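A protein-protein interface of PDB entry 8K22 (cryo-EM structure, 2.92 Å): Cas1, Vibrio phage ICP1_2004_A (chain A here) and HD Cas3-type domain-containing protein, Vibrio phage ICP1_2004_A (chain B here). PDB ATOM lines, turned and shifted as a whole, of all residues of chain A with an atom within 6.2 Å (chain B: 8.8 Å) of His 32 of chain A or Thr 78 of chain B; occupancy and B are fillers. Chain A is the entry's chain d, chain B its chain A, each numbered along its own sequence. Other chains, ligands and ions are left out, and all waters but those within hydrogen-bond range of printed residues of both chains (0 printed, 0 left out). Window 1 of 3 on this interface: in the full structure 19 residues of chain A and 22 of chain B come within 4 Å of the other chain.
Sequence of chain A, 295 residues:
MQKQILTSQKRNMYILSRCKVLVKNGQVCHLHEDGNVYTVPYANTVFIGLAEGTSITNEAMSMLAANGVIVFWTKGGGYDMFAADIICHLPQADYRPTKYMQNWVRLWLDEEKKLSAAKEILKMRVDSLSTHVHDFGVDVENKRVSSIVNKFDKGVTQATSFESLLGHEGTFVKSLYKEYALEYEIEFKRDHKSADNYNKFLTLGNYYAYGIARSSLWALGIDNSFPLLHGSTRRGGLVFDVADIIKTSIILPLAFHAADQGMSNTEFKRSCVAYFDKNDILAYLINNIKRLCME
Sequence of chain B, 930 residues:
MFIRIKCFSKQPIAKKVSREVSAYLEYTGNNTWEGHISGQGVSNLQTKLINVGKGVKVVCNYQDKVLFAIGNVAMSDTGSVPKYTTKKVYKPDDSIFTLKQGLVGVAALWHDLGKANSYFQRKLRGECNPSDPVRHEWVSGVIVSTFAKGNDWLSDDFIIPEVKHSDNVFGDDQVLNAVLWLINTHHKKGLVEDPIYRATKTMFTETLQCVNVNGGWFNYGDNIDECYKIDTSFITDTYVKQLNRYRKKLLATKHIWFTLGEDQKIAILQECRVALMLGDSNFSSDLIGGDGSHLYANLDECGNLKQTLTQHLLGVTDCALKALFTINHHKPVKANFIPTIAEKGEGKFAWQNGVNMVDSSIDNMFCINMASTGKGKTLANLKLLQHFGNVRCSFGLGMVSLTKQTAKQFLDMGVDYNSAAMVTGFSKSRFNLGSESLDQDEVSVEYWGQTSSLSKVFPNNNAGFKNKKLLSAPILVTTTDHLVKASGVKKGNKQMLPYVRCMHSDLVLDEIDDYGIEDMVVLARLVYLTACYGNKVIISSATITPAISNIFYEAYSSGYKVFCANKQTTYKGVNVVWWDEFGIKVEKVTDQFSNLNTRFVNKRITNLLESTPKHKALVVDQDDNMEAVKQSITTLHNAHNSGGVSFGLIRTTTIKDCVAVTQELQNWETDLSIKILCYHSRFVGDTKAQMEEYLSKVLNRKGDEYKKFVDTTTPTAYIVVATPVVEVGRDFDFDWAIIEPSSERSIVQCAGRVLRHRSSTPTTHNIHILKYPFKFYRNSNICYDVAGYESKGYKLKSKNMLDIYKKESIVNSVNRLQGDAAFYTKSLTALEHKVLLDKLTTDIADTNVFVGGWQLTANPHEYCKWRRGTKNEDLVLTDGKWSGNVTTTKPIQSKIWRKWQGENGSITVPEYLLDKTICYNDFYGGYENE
Among the printed residues, merely in contact across the chains: Tyr 38 of chain A with Ser 80 of chain B, Val 37 of chain A with Pro 82 of chain B, Tyr 38 of chain A with Val 81 of chain B, Asn 36 of chain A with Ala 74 of chain B, Asn 36 of chain A with Pro 82 of chain B, His 32 of chain A with Thr 78 of chain B, Tyr 38 of chain A with Pro 82 of chain B, Tyr 38 of chain A with Asp 77 of chain B, Tyr 38 of chain A with Ser 76 of chain B, Glu 33 of chain A with Val 89 of chain B, Asn 36 of chain A with Thr 85 of chain B, Asp 34 of chain A with Asp 77 of chain B, Gly 35 of chain A with Val 89 of chain B and Asn 36 of chain A with Met 75 of chain B.
OH of Tyr 38 of chain A is in hydrogen-bond range of O of Gly 79 of chain B. The guanidinium group (NH1) of Arg 270 of chain A lies within salt-bridge range of the side-chain carboxylate (OD2) of Asp 64 of chain B, 2.5 Å away. The side-chain hydroxyl (OH) of Tyr 38 of chain A lies within hydrogen-bond range of the backbone carbonyl oxygen (O) of Met 75 of chain B (2.7 Å). The backbone carbonyl oxygen (O) of Gly 35 of chain A lies close to the side-chain hydroxyl (OG1) of Thr 85 of chain B (2.4 Å).
The backbone carbonyl oxygen (O) of Gly 79 of chain B lies within hydrogen-bond range of the side-chain hydroxyl (OG) of Ser 76 of chain B, 2.9 Å away. OD1 of Asp 34 of chain A sits at hydrogen-bond distance from ND2 of Asn 36 of chain A, at 3.1 Å. NH2 of Arg 270 of chain A lies within hydrogen-bond range of OG1 of Thr 266 of chain A (3.1 Å). N of His 30 of chain A is in hydrogen-bond range of O of Tyr 38 of chain A. The backbone carbonyl oxygen (O) of Met 75 of chain B sits at hydrogen-bond distance from the backbone NH (N) of Val 81 of chain B. A ring nitrogen (NE2) of His 32 of chain A lies within hydrogen-bond range of the backbone carbonyl oxygen (O) of Ser 17 of chain A, 3.5 Å away.
Of the 14 printed residues of chain B, 12 touch a printed residue of chain A. Hydrophobic or aromatic side chains of chain B that line the printed part of chain A: Ala 74, Pro 82 and Val 89. Among the printed residues, 18 pairs touch across the chains. Among the printed residues, Asp or Glu carboxylates within 4 Å of a Lys or Arg side-chain nitrogen of the other chain: Arg 270 of chain A with Asp 64 of chain B (2.5 Å).
Arg 18 of chain A touches none of the printed residues of chain B. Of chain B, only Thr 78 (3.5 Å) comes within 4 Å of His 32 of chain A. Of the printed residues of chain B, Asp 34 of chain A touches Asp 77. Of the printed residues of chain B, Val 37 of chain A touches Pro 82 (3.3 Å). Of the printed residues of chain B, Arg 270 of chain A touches Asp 64. Of chain A, only His 32 comes within 4 Å of Thr 78 of chain B. Of the printed residues of chain A, Thr 85 of chain B touches Gly 35 and Asn 36. The nearest residue of chain B that does not touch His 32 of chain A is Asp 77 of chain B (4.1 Å). The nearest residue of chain A that does not touch Thr 78 of chain B is Thr 266 of chain A (4.6 Å).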
ATOM      1  N   SER A  17      15.239 -20.677  32.971  1.00  0.00           N
ATOM      2  CA  SER A  17      14.391 -19.501  33.100  1.00  0.00           C
ATOM      3  C   SER A  17      14.494 -18.651  31.845  1.00  0.00           C
ATOM      4  O   SER A  17      15.600 -18.262  31.451  1.00  0.00           O
ATOM      5  CB  SER A  17      14.797 -18.671  34.323  1.00  0.00           C
ATOM      6  OG  SER A  17      14.528 -19.362  35.530  1.00  0.00           O
ATOM      7  N   ARG A  18      13.337 -18.366  31.236  1.00  0.00           N
ATOM      8  CA  ARG A  18      13.164 -17.450  30.103  1.00  0.00           C
ATOM      9  C   ARG A  18      14.030 -17.886  28.912  1.00  0.00           C
ATOM     10  O   ARG A  18      14.922 -17.177  28.439  1.00  0.00           O
ATOM     11  CB  ARG A  18      13.446 -16.004  30.540  1.00  0.00           C
ATOM     12  CG  ARG A  18      13.002 -14.912  29.561  1.00  0.00           C
ATOM     13  CD  ARG A  18      12.471 -13.661  30.272  1.00  0.00           C
ATOM     14  NE  ARG A  18      11.725 -13.908  31.504  1.00  0.00           N
ATOM     15  CZ  ARG A  18      10.520 -14.461  31.582  1.00  0.00           C
ATOM     16  NH1 ARG A  18       9.835 -14.795  30.499  1.00  0.00           N
ATOM     17  NH2 ARG A  18       9.978 -14.664  32.779  1.00  0.00           N
ATOM     18  N   CYS A  19      13.752 -19.107  28.462  1.00  0.00           N
ATOM     19  CA  CYS A  19      14.479 -19.724  27.362  1.00  0.00           C
ATOM     20  C   CYS A  19      13.666 -20.895  26.841  1.00  0.00           C
ATOM     21  O   CYS A  19      13.050 -21.636  27.610  1.00  0.00           O
ATOM     22  CB  CYS A  19      15.870 -20.196  27.795  1.00  0.00           C
ATOM     23  SG  CYS A  19      15.856 -21.297  29.222  1.00  0.00           S
ATOM     24  N   LYS A  20      13.669 -21.057  25.523  1.00  0.00           N
ATOM     25  CA  LYS A  20      12.976 -22.168  24.888  1.00  0.00           C
ATOM     26  C   LYS A  20      13.983 -23.308  24.767  1.00  0.00           C
ATOM     27  O   LYS A  20      15.095 -23.118  24.267  1.00  0.00           O
ATOM     28  CB  LYS A  20      12.369 -21.764  23.542  1.00  0.00           C
ATOM     29  CG  LYS A  20      12.547 -22.759  22.395  1.00  0.00           C
ATOM     30  CD  LYS A  20      12.180 -22.147  21.056  1.00  0.00           C
ATOM     31  CE  LYS A  20      13.058 -20.963  20.744  1.00  0.00           C
ATOM     32  NZ  LYS A  20      14.470 -21.349  20.863  1.00  0.00           N
ATOM     33  N   HIS A  30      19.268 -24.917  25.691  1.00  0.00           N
ATOM     34  CA  HIS A  30      18.213 -23.929  25.855  1.00  0.00           C
ATOM     35  C   HIS A  30      18.652 -22.631  25.201  1.00  0.00           C
ATOM     36  O   HIS A  30      19.807 -22.217  25.341  1.00  0.00           O
ATOM     37  CB  HIS A  30      17.860 -23.707  27.329  1.00  0.00           C
ATOM     38  CG  HIS A  30      19.042 -23.574  28.235  1.00  0.00           C
ATOM     39  ND1 HIS A  30      19.710 -24.663  28.749  1.00  0.00           N
ATOM     40  CD2 HIS A  30      19.658 -22.483  28.746  1.00  0.00           C
ATOM     41  CE1 HIS A  30      20.695 -24.250  29.525  1.00  0.00           C
ATOM     42  NE2 HIS A  30      20.683 -22.931  29.543  1.00  0.00           N
ATOM     43  N   LEU A  31      17.726 -22.010  24.479  1.00  0.00           N
ATOM     44  CA  LEU A  31      17.956 -20.785  23.732  1.00  0.00           C
ATOM     45  C   LEU A  31      17.159 -19.658  24.373  1.00  0.00           C
ATOM     46  O   LEU A  31      15.925 -19.693  24.377  1.00  0.00           O
ATOM     47  CB  LEU A  31      17.562 -20.993  22.267  1.00  0.00           C
ATOM     48  CG  LEU A  31      17.531 -19.859  21.239  1.00  0.00           C
ATOM     49  CD1 LEU A  31      18.723 -18.966  21.343  1.00  0.00           C
ATOM     50  CD2 LEU A  31      17.500 -20.458  19.846  1.00  0.00           C
ATOM     51  N   HIS A  32      17.860 -18.669  24.923  1.00  0.00           N
ATOM     52  CA  HIS A  32      17.199 -17.524  25.527  1.00  0.00           C
ATOM     53  C   HIS A  32      16.723 -16.548  24.458  1.00  0.00           C
ATOM     54  O   HIS A  32      16.957 -16.727  23.260  1.00  0.00           O
ATOM     55  CB  HIS A  32      18.127 -16.805  26.504  1.00  0.00           C
ATOM     56  CG  HIS A  32      18.443 -17.590  27.736  1.00  0.00           C
ATOM     57  ND1 HIS A  32      19.191 -18.747  27.716  1.00  0.00           N
ATOM     58  CD2 HIS A  32      18.096 -17.389  29.028  1.00  0.00           C
ATOM     59  CE1 HIS A  32      19.304 -19.214  28.946  1.00  0.00           C
ATOM     60  NE2 HIS A  32      18.646 -18.410  29.761  1.00  0.00           N
ATOM     61  N   GLU A  33      16.058 -15.486  24.906  1.00  0.00           N
ATOM     62  CA  GLU A  33      15.549 -14.470  23.984  1.00  0.00           C
ATOM     63  C   GLU A  33      16.573 -13.365  23.739  1.00  0.00           C
ATOM     64  O   GLU A  33      16.274 -12.175  23.815  1.00  0.00           O
ATOM     65  CB  GLU A  33      14.243 -13.894  24.516  1.00  0.00           C
ATOM     66  CG  GLU A  33      14.179 -13.783  26.028  1.00  0.00           C
ATOM     67  CD  GLU A  33      12.929 -13.071  26.506  1.00  0.00           C
ATOM     68  OE1 GLU A  33      11.815 -13.527  26.169  1.00  0.00           O
ATOM     69  OE2 GLU A  33      13.061 -12.054  27.218  1.00  0.00           O
ATOM     70  N   ASP A  34      17.806 -13.773  23.441  1.00  0.00           N
ATOM     71  CA  ASP A  34      18.814 -12.878  22.893  1.00  0.00           C
ATOM     72  C   ASP A  34      19.718 -13.597  21.901  1.00  0.00           C
ATOM     73  O   ASP A  34      20.663 -12.983  21.389  1.00  0.00           O
ATOM     74  CB  ASP A  34      19.650 -12.238  24.009  1.00  0.00           C
ATOM     75  CG  ASP A  34      19.965 -13.205  25.129  1.00  0.00           C
ATOM     76  OD1 ASP A  34      20.458 -14.313  24.844  1.00  0.00           O
ATOM     77  OD2 ASP A  34      19.724 -12.849  26.302  1.00  0.00           O
ATOM     78  N   GLY A  35      19.459 -14.870  21.615  1.00  0.00           N
ATOM     79  CA  GLY A  35      20.269 -15.643  20.704  1.00  0.00           C
ATOM     80  C   GLY A  35      21.250 -16.588  21.363  1.00  0.00           C
ATOM     81  O   GLY A  35      21.986 -17.281  20.649  1.00  0.00           O
ATOM     82  N   ASN A  36      21.272 -16.661  22.689  1.00  0.00           N
ATOM     83  CA  ASN A  36      22.266 -17.469  23.380  1.00  0.00           C
ATOM     84  C   ASN A  36      21.787 -18.905  23.558  1.00  0.00           C
ATOM     85  O   ASN A  36      20.741 -19.145  24.162  1.00  0.00           O
ATOM     86  CB  ASN A  36      22.586 -16.850  24.737  1.00  0.00           C
ATOM     87  CG  ASN A  36      23.352 -15.553  24.613  1.00  0.00           C
ATOM     88  OD1 ASN A  36      23.934 -15.261  23.569  1.00  0.00           O
ATOM     89  ND2 ASN A  36      23.358 -14.765  25.681  1.00  0.00           N
ATOM     90  N   VAL A  37      22.576 -19.860  23.065  1.00  0.00           N
ATOM     91  CA  VAL A  37      22.257 -21.284  23.128  1.00  0.00           C
ATOM     92  C   VAL A  37      23.229 -21.952  24.090  1.00  0.00           C
ATOM     93  O   VAL A  37      24.408 -22.126  23.760  1.00  0.00           O
ATOM     94  CB  VAL A  37      22.354 -21.950  21.747  1.00  0.00           C
ATOM     95  CG1 VAL A  37      21.873 -23.389  21.815  1.00  0.00           C
ATOM     96  CG2 VAL A  37      21.605 -21.157  20.696  1.00  0.00           C
ATOM     97  N   TYR A  38      22.737 -22.366  25.255  1.00  0.00           N
ATOM     98  CA  TYR A  38      23.557 -23.053  26.248  1.00  0.00           C
ATOM     99  C   TYR A  38      23.162 -24.521  26.316  1.00  0.00           C
ATOM    100  O   TYR A  38      21.988 -24.838  26.512  1.00  0.00           O
ATOM    101  CB  TYR A  38      23.411 -22.413  27.630  1.00  0.00           C
ATOM    102  CG  TYR A  38      23.623 -20.922  27.658  1.00  0.00           C
ATOM    103  CD1 TYR A  38      24.895 -20.382  27.529  1.00  0.00           C
ATOM    104  CD2 TYR A  38      22.553 -20.053  27.821  1.00  0.00           C
ATOM    105  CE1 TYR A  38      25.096 -19.017  27.561  1.00  0.00           C
ATOM    106  CE2 TYR A  38      22.743 -18.687  27.851  1.00  0.00           C
ATOM    107  CZ  TYR A  38      24.016 -18.175  27.720  1.00  0.00           C
ATOM    108  OH  TYR A  38      24.212 -16.814  27.749  1.00  0.00           O
ATOM    109  N   THR A 266      21.866 -17.166  40.556  1.00  0.00           N
ATOM    110  CA  THR A 266      22.729 -18.188  39.969  1.00  0.00           C
ATOM    111  C   THR A 266      23.718 -18.754  40.982  1.00  0.00           C
ATOM    112  O   THR A 266      24.069 -19.940  40.911  1.00  0.00           O
ATOM    113  CB  THR A 266      23.469 -17.621  38.757  1.00  0.00           C
ATOM    114  OG1 THR A 266      24.628 -16.902  39.193  1.00  0.00           O
ATOM    115  CG2 THR A 266      22.561 -16.701  37.955  1.00  0.00           C
ATOM    116  N   ARG A 270      24.004 -22.730  41.895  1.00  0.00           N
ATOM    117  CA  ARG A 270      25.292 -23.407  41.960  1.00  0.00           C
ATOM    118  C   ARG A 270      25.620 -23.900  43.365  1.00  0.00           C
ATOM    119  O   ARG A 270      26.273 -24.937  43.514  1.00  0.00           O
ATOM    120  CB  ARG A 270      26.349 -22.449  41.435  1.00  0.00           C
ATOM    121  CG  ARG A 270      27.626 -23.040  40.888  1.00  0.00           C
ATOM    122  CD  ARG A 270      28.343 -22.140  39.833  1.00  0.00           C
ATOM    123  NE  ARG A 270      27.515 -21.254  39.006  1.00  0.00           N
ATOM    124  CZ  ARG A 270      27.169 -20.001  39.289  1.00  0.00           C
ATOM    125  NH1 ARG A 270      27.428 -19.460  40.466  1.00  0.00           N
ATOM    126  NH2 ARG A 270      26.505 -19.293  38.380  1.00  0.00           N
ATOM    127  N   ASP B  64      32.114 -16.337  40.097  1.00  0.00           N
ATOM    128  CA  ASP B  64      31.084 -16.727  39.149  1.00  0.00           C
ATOM    129  C   ASP B  64      30.274 -15.558  38.603  1.00  0.00           C
ATOM    130  O   ASP B  64      29.609 -15.718  37.574  1.00  0.00           O
ATOM    131  CB  ASP B  64      30.148 -17.749  39.790  1.00  0.00           C
ATOM    132  CG  ASP B  64      29.875 -17.453  41.251  1.00  0.00           C
ATOM    133  OD1 ASP B  64      30.394 -16.442  41.759  1.00  0.00           O
ATOM    134  OD2 ASP B  64      29.135 -18.232  41.888  1.00  0.00           O
ATOM    135  N   ALA B  74      26.785 -10.737  24.150  1.00  0.00           N
ATOM    136  CA  ALA B  74      25.623 -11.169  24.917  1.00  0.00           C
ATOM    137  C   ALA B  74      26.080 -11.950  26.133  1.00  0.00           C
ATOM    138  O   ALA B  74      25.457 -11.836  27.188  1.00  0.00           O
ATOM    139  CB  ALA B  74      24.698 -11.995  24.047  1.00  0.00           C
ATOM    140  N   MET B  75      27.140 -12.746  25.993  1.00  0.00           N
ATOM    141  CA  MET B  75      27.730 -13.474  27.127  1.00  0.00           C
ATOM    142  C   MET B  75      26.801 -14.256  28.036  1.00  0.00           C
ATOM    143  O   MET B  75      26.529 -15.425  27.778  1.00  0.00           O
ATOM    144  CB  MET B  75      28.591 -12.529  27.976  1.00  0.00           C
ATOM    145  N   SER B  76      26.331 -13.627  29.110  1.00  0.00           N
ATOM    146  CA  SER B  76      25.519 -14.349  30.080  1.00  0.00           C
ATOM    147  C   SER B  76      24.172 -13.755  30.452  1.00  0.00           C
ATOM    148  O   SER B  76      24.110 -12.607  30.890  1.00  0.00           O
ATOM    149  CB  SER B  76      26.323 -14.530  31.371  1.00  0.00           C
ATOM    150  OG  SER B  76      25.566 -15.232  32.341  1.00  0.00           O
ATOM    151  N   ASP B  77      23.093 -14.521  30.291  1.00  0.00           N
ATOM    152  CA  ASP B  77      21.801 -14.060  30.754  1.00  0.00           C
ATOM    153  C   ASP B  77      21.569 -14.972  31.930  1.00  0.00           C
ATOM    154  O   ASP B  77      21.110 -14.533  32.984  1.00  0.00           O
ATOM    155  CB  ASP B  77      20.749 -14.305  29.691  1.00  0.00           C
ATOM    156  N   THR B  78      21.889 -16.251  31.758  1.00  0.00           N
ATOM    157  CA  THR B  78      21.771 -17.209  32.852  1.00  0.00           C
ATOM    158  C   THR B  78      23.052 -18.006  32.829  1.00  0.00           C
ATOM    159  O   THR B  78      23.856 -17.925  33.755  1.00  0.00           O
ATOM    160  CB  THR B  78      20.572 -18.153  32.671  1.00  0.00           C
ATOM    161  N   GLY B  79      23.265 -18.765  31.761  1.00  0.00           N
ATOM    162  CA  GLY B  79      24.513 -19.483  31.624  1.00  0.00           C
ATOM    163  C   GLY B  79      25.427 -18.530  30.902  1.00  0.00           C
ATOM    164  O   GLY B  79      24.999 -17.466  30.503  1.00  0.00           O
ATOM    165  N   SER B  80      26.680 -18.905  30.716  1.00  0.00           N
ATOM    166  CA  SER B  80      27.599 -18.056  29.973  1.00  0.00           C
ATOM    167  C   SER B  80      28.110 -18.785  28.748  1.00  0.00           C
ATOM    168  O   SER B  80      28.092 -20.016  28.740  1.00  0.00           O
ATOM    169  CB  SER B  80      28.761 -17.603  30.856  1.00  0.00           C
ATOM    170  OG  SER B  80      29.331 -16.402  30.365  1.00  0.00           O
ATOM    171  N   VAL B  81      28.551 -18.046  27.727  1.00  0.00           N
ATOM    172  CA  VAL B  81      29.044 -18.629  26.475  1.00  0.00           C
ATOM    173  C   VAL B  81      27.999 -19.421  25.718  1.00  0.00           C
ATOM    174  O   VAL B  81      27.823 -20.617  25.923  1.00  0.00           O
ATOM    175  CB  VAL B  81      30.358 -19.436  26.615  1.00  0.00           C
ATOM    176  CG1 VAL B  81      30.971 -19.692  25.246  1.00  0.00           C
ATOM    177  CG2 VAL B  81      31.357 -18.707  27.504  1.00  0.00           C
ATOM    178  N   PRO B  82      27.309 -18.756  24.810  1.00  0.00           N
ATOM    179  CA  PRO B  82      26.321 -19.444  23.994  1.00  0.00           C
ATOM    180  C   PRO B  82      26.887 -20.225  22.852  1.00  0.00           C
ATOM    181  O   PRO B  82      28.096 -20.325  22.691  1.00  0.00           O
ATOM    182  CB  PRO B  82      25.616 -18.293  23.350  1.00  0.00           C
ATOM    183  CG  PRO B  82      26.665 -17.266  23.187  1.00  0.00           C
ATOM    184  CD  PRO B  82      27.367 -17.322  24.500  1.00  0.00           C
ATOM    185  N   THR B  85      24.725 -17.729  17.624  1.00  0.00           N
ATOM    186  CA  THR B  85      23.623 -16.785  17.629  1.00  0.00           C
ATOM    187  C   THR B  85      23.462 -16.288  16.204  1.00  0.00           C
ATOM    188  O   THR B  85      24.400 -15.712  15.645  1.00  0.00           O
ATOM    189  CB  THR B  85      23.934 -15.622  18.565  1.00  0.00           C
ATOM    190  OG1 THR B  85      23.935 -16.090  19.917  1.00  0.00           O
ATOM    191  CG2 THR B  85      22.917 -14.505  18.400  1.00  0.00           C
ATOM    192  N   LYS B  88      16.607 -13.762  13.995  1.00  0.00           N
ATOM    193  CA  LYS B  88      15.168 -14.041  14.100  1.00  0.00           C
ATOM    194  C   LYS B  88      14.805 -14.729  15.419  1.00  0.00           C
ATOM    195  O   LYS B  88      14.348 -15.874  15.451  1.00  0.00           O
ATOM    196  CB  LYS B  88      14.666 -14.856  12.902  1.00  0.00           C
ATOM    197  CG  LYS B  88      14.895 -14.195  11.558  1.00  0.00           C
ATOM    198  CD  LYS B  88      15.498 -15.165  10.562  1.00  0.00           C
ATOM    199  CE  LYS B  88      15.917 -14.443   9.293  1.00  0.00           C
ATOM    200  NZ  LYS B  88      16.729 -15.309   8.393  1.00  0.00           N
ATOM    201  N   VAL B  89      15.021 -14.006  16.510  1.00  0.00           N
ATOM    202  CA  VAL B  89      14.782 -14.553  17.841  1.00  0.00           C
ATOM    203  C   VAL B  89      13.324 -14.408  18.251  1.00  0.00           C
ATOM    204  O   VAL B  89      12.652 -15.392  18.570  1.00  0.00           O
ATOM    205  CB  VAL B  89      15.718 -13.874  18.864  1.00  0.00           C
ATOM    206  CG1 VAL B  89      15.326 -14.271  20.273  1.00  0.00           C
ATOM    207  CG2 VAL B  89      17.164 -14.237  18.583  1.00  0.00           C
ATOM    208  N   TYR B  90      12.806 -13.182  18.254  1.00  0.00           N
ATOM    209  CA  TYR B  90      11.505 -12.890  18.844  1.00  0.00           C
ATOM    210  C   TYR B  90      10.453 -12.409  17.848  1.00  0.00           C
ATOM    211  O   TYR B  90       9.395 -13.041  17.773  1.00  0.00           O
ATOM    212  CB  TYR B  90      11.740 -11.957  20.057  1.00  0.00           C
ATOM    213  CG  TYR B  90      12.517 -10.664  19.822  1.00  0.00           C
ATOM    214  CD1 TYR B  90      11.928  -9.534  19.299  1.00  0.00           C
ATOM    215  CD2 TYR B  90      13.843 -10.580  20.226  1.00  0.00           C
ATOM    216  CE1 TYR B  90      12.650  -8.365  19.106  1.00  0.00           C
ATOM    217  CE2 TYR B  90      14.574  -9.423  20.048  1.00  0.00           C
ATOM    218  CZ  TYR B  90      13.973  -8.316  19.489  1.00  0.00           C
ATOM    219  OH  TYR B  90      14.695  -7.161  19.317  1.00  0.00           O
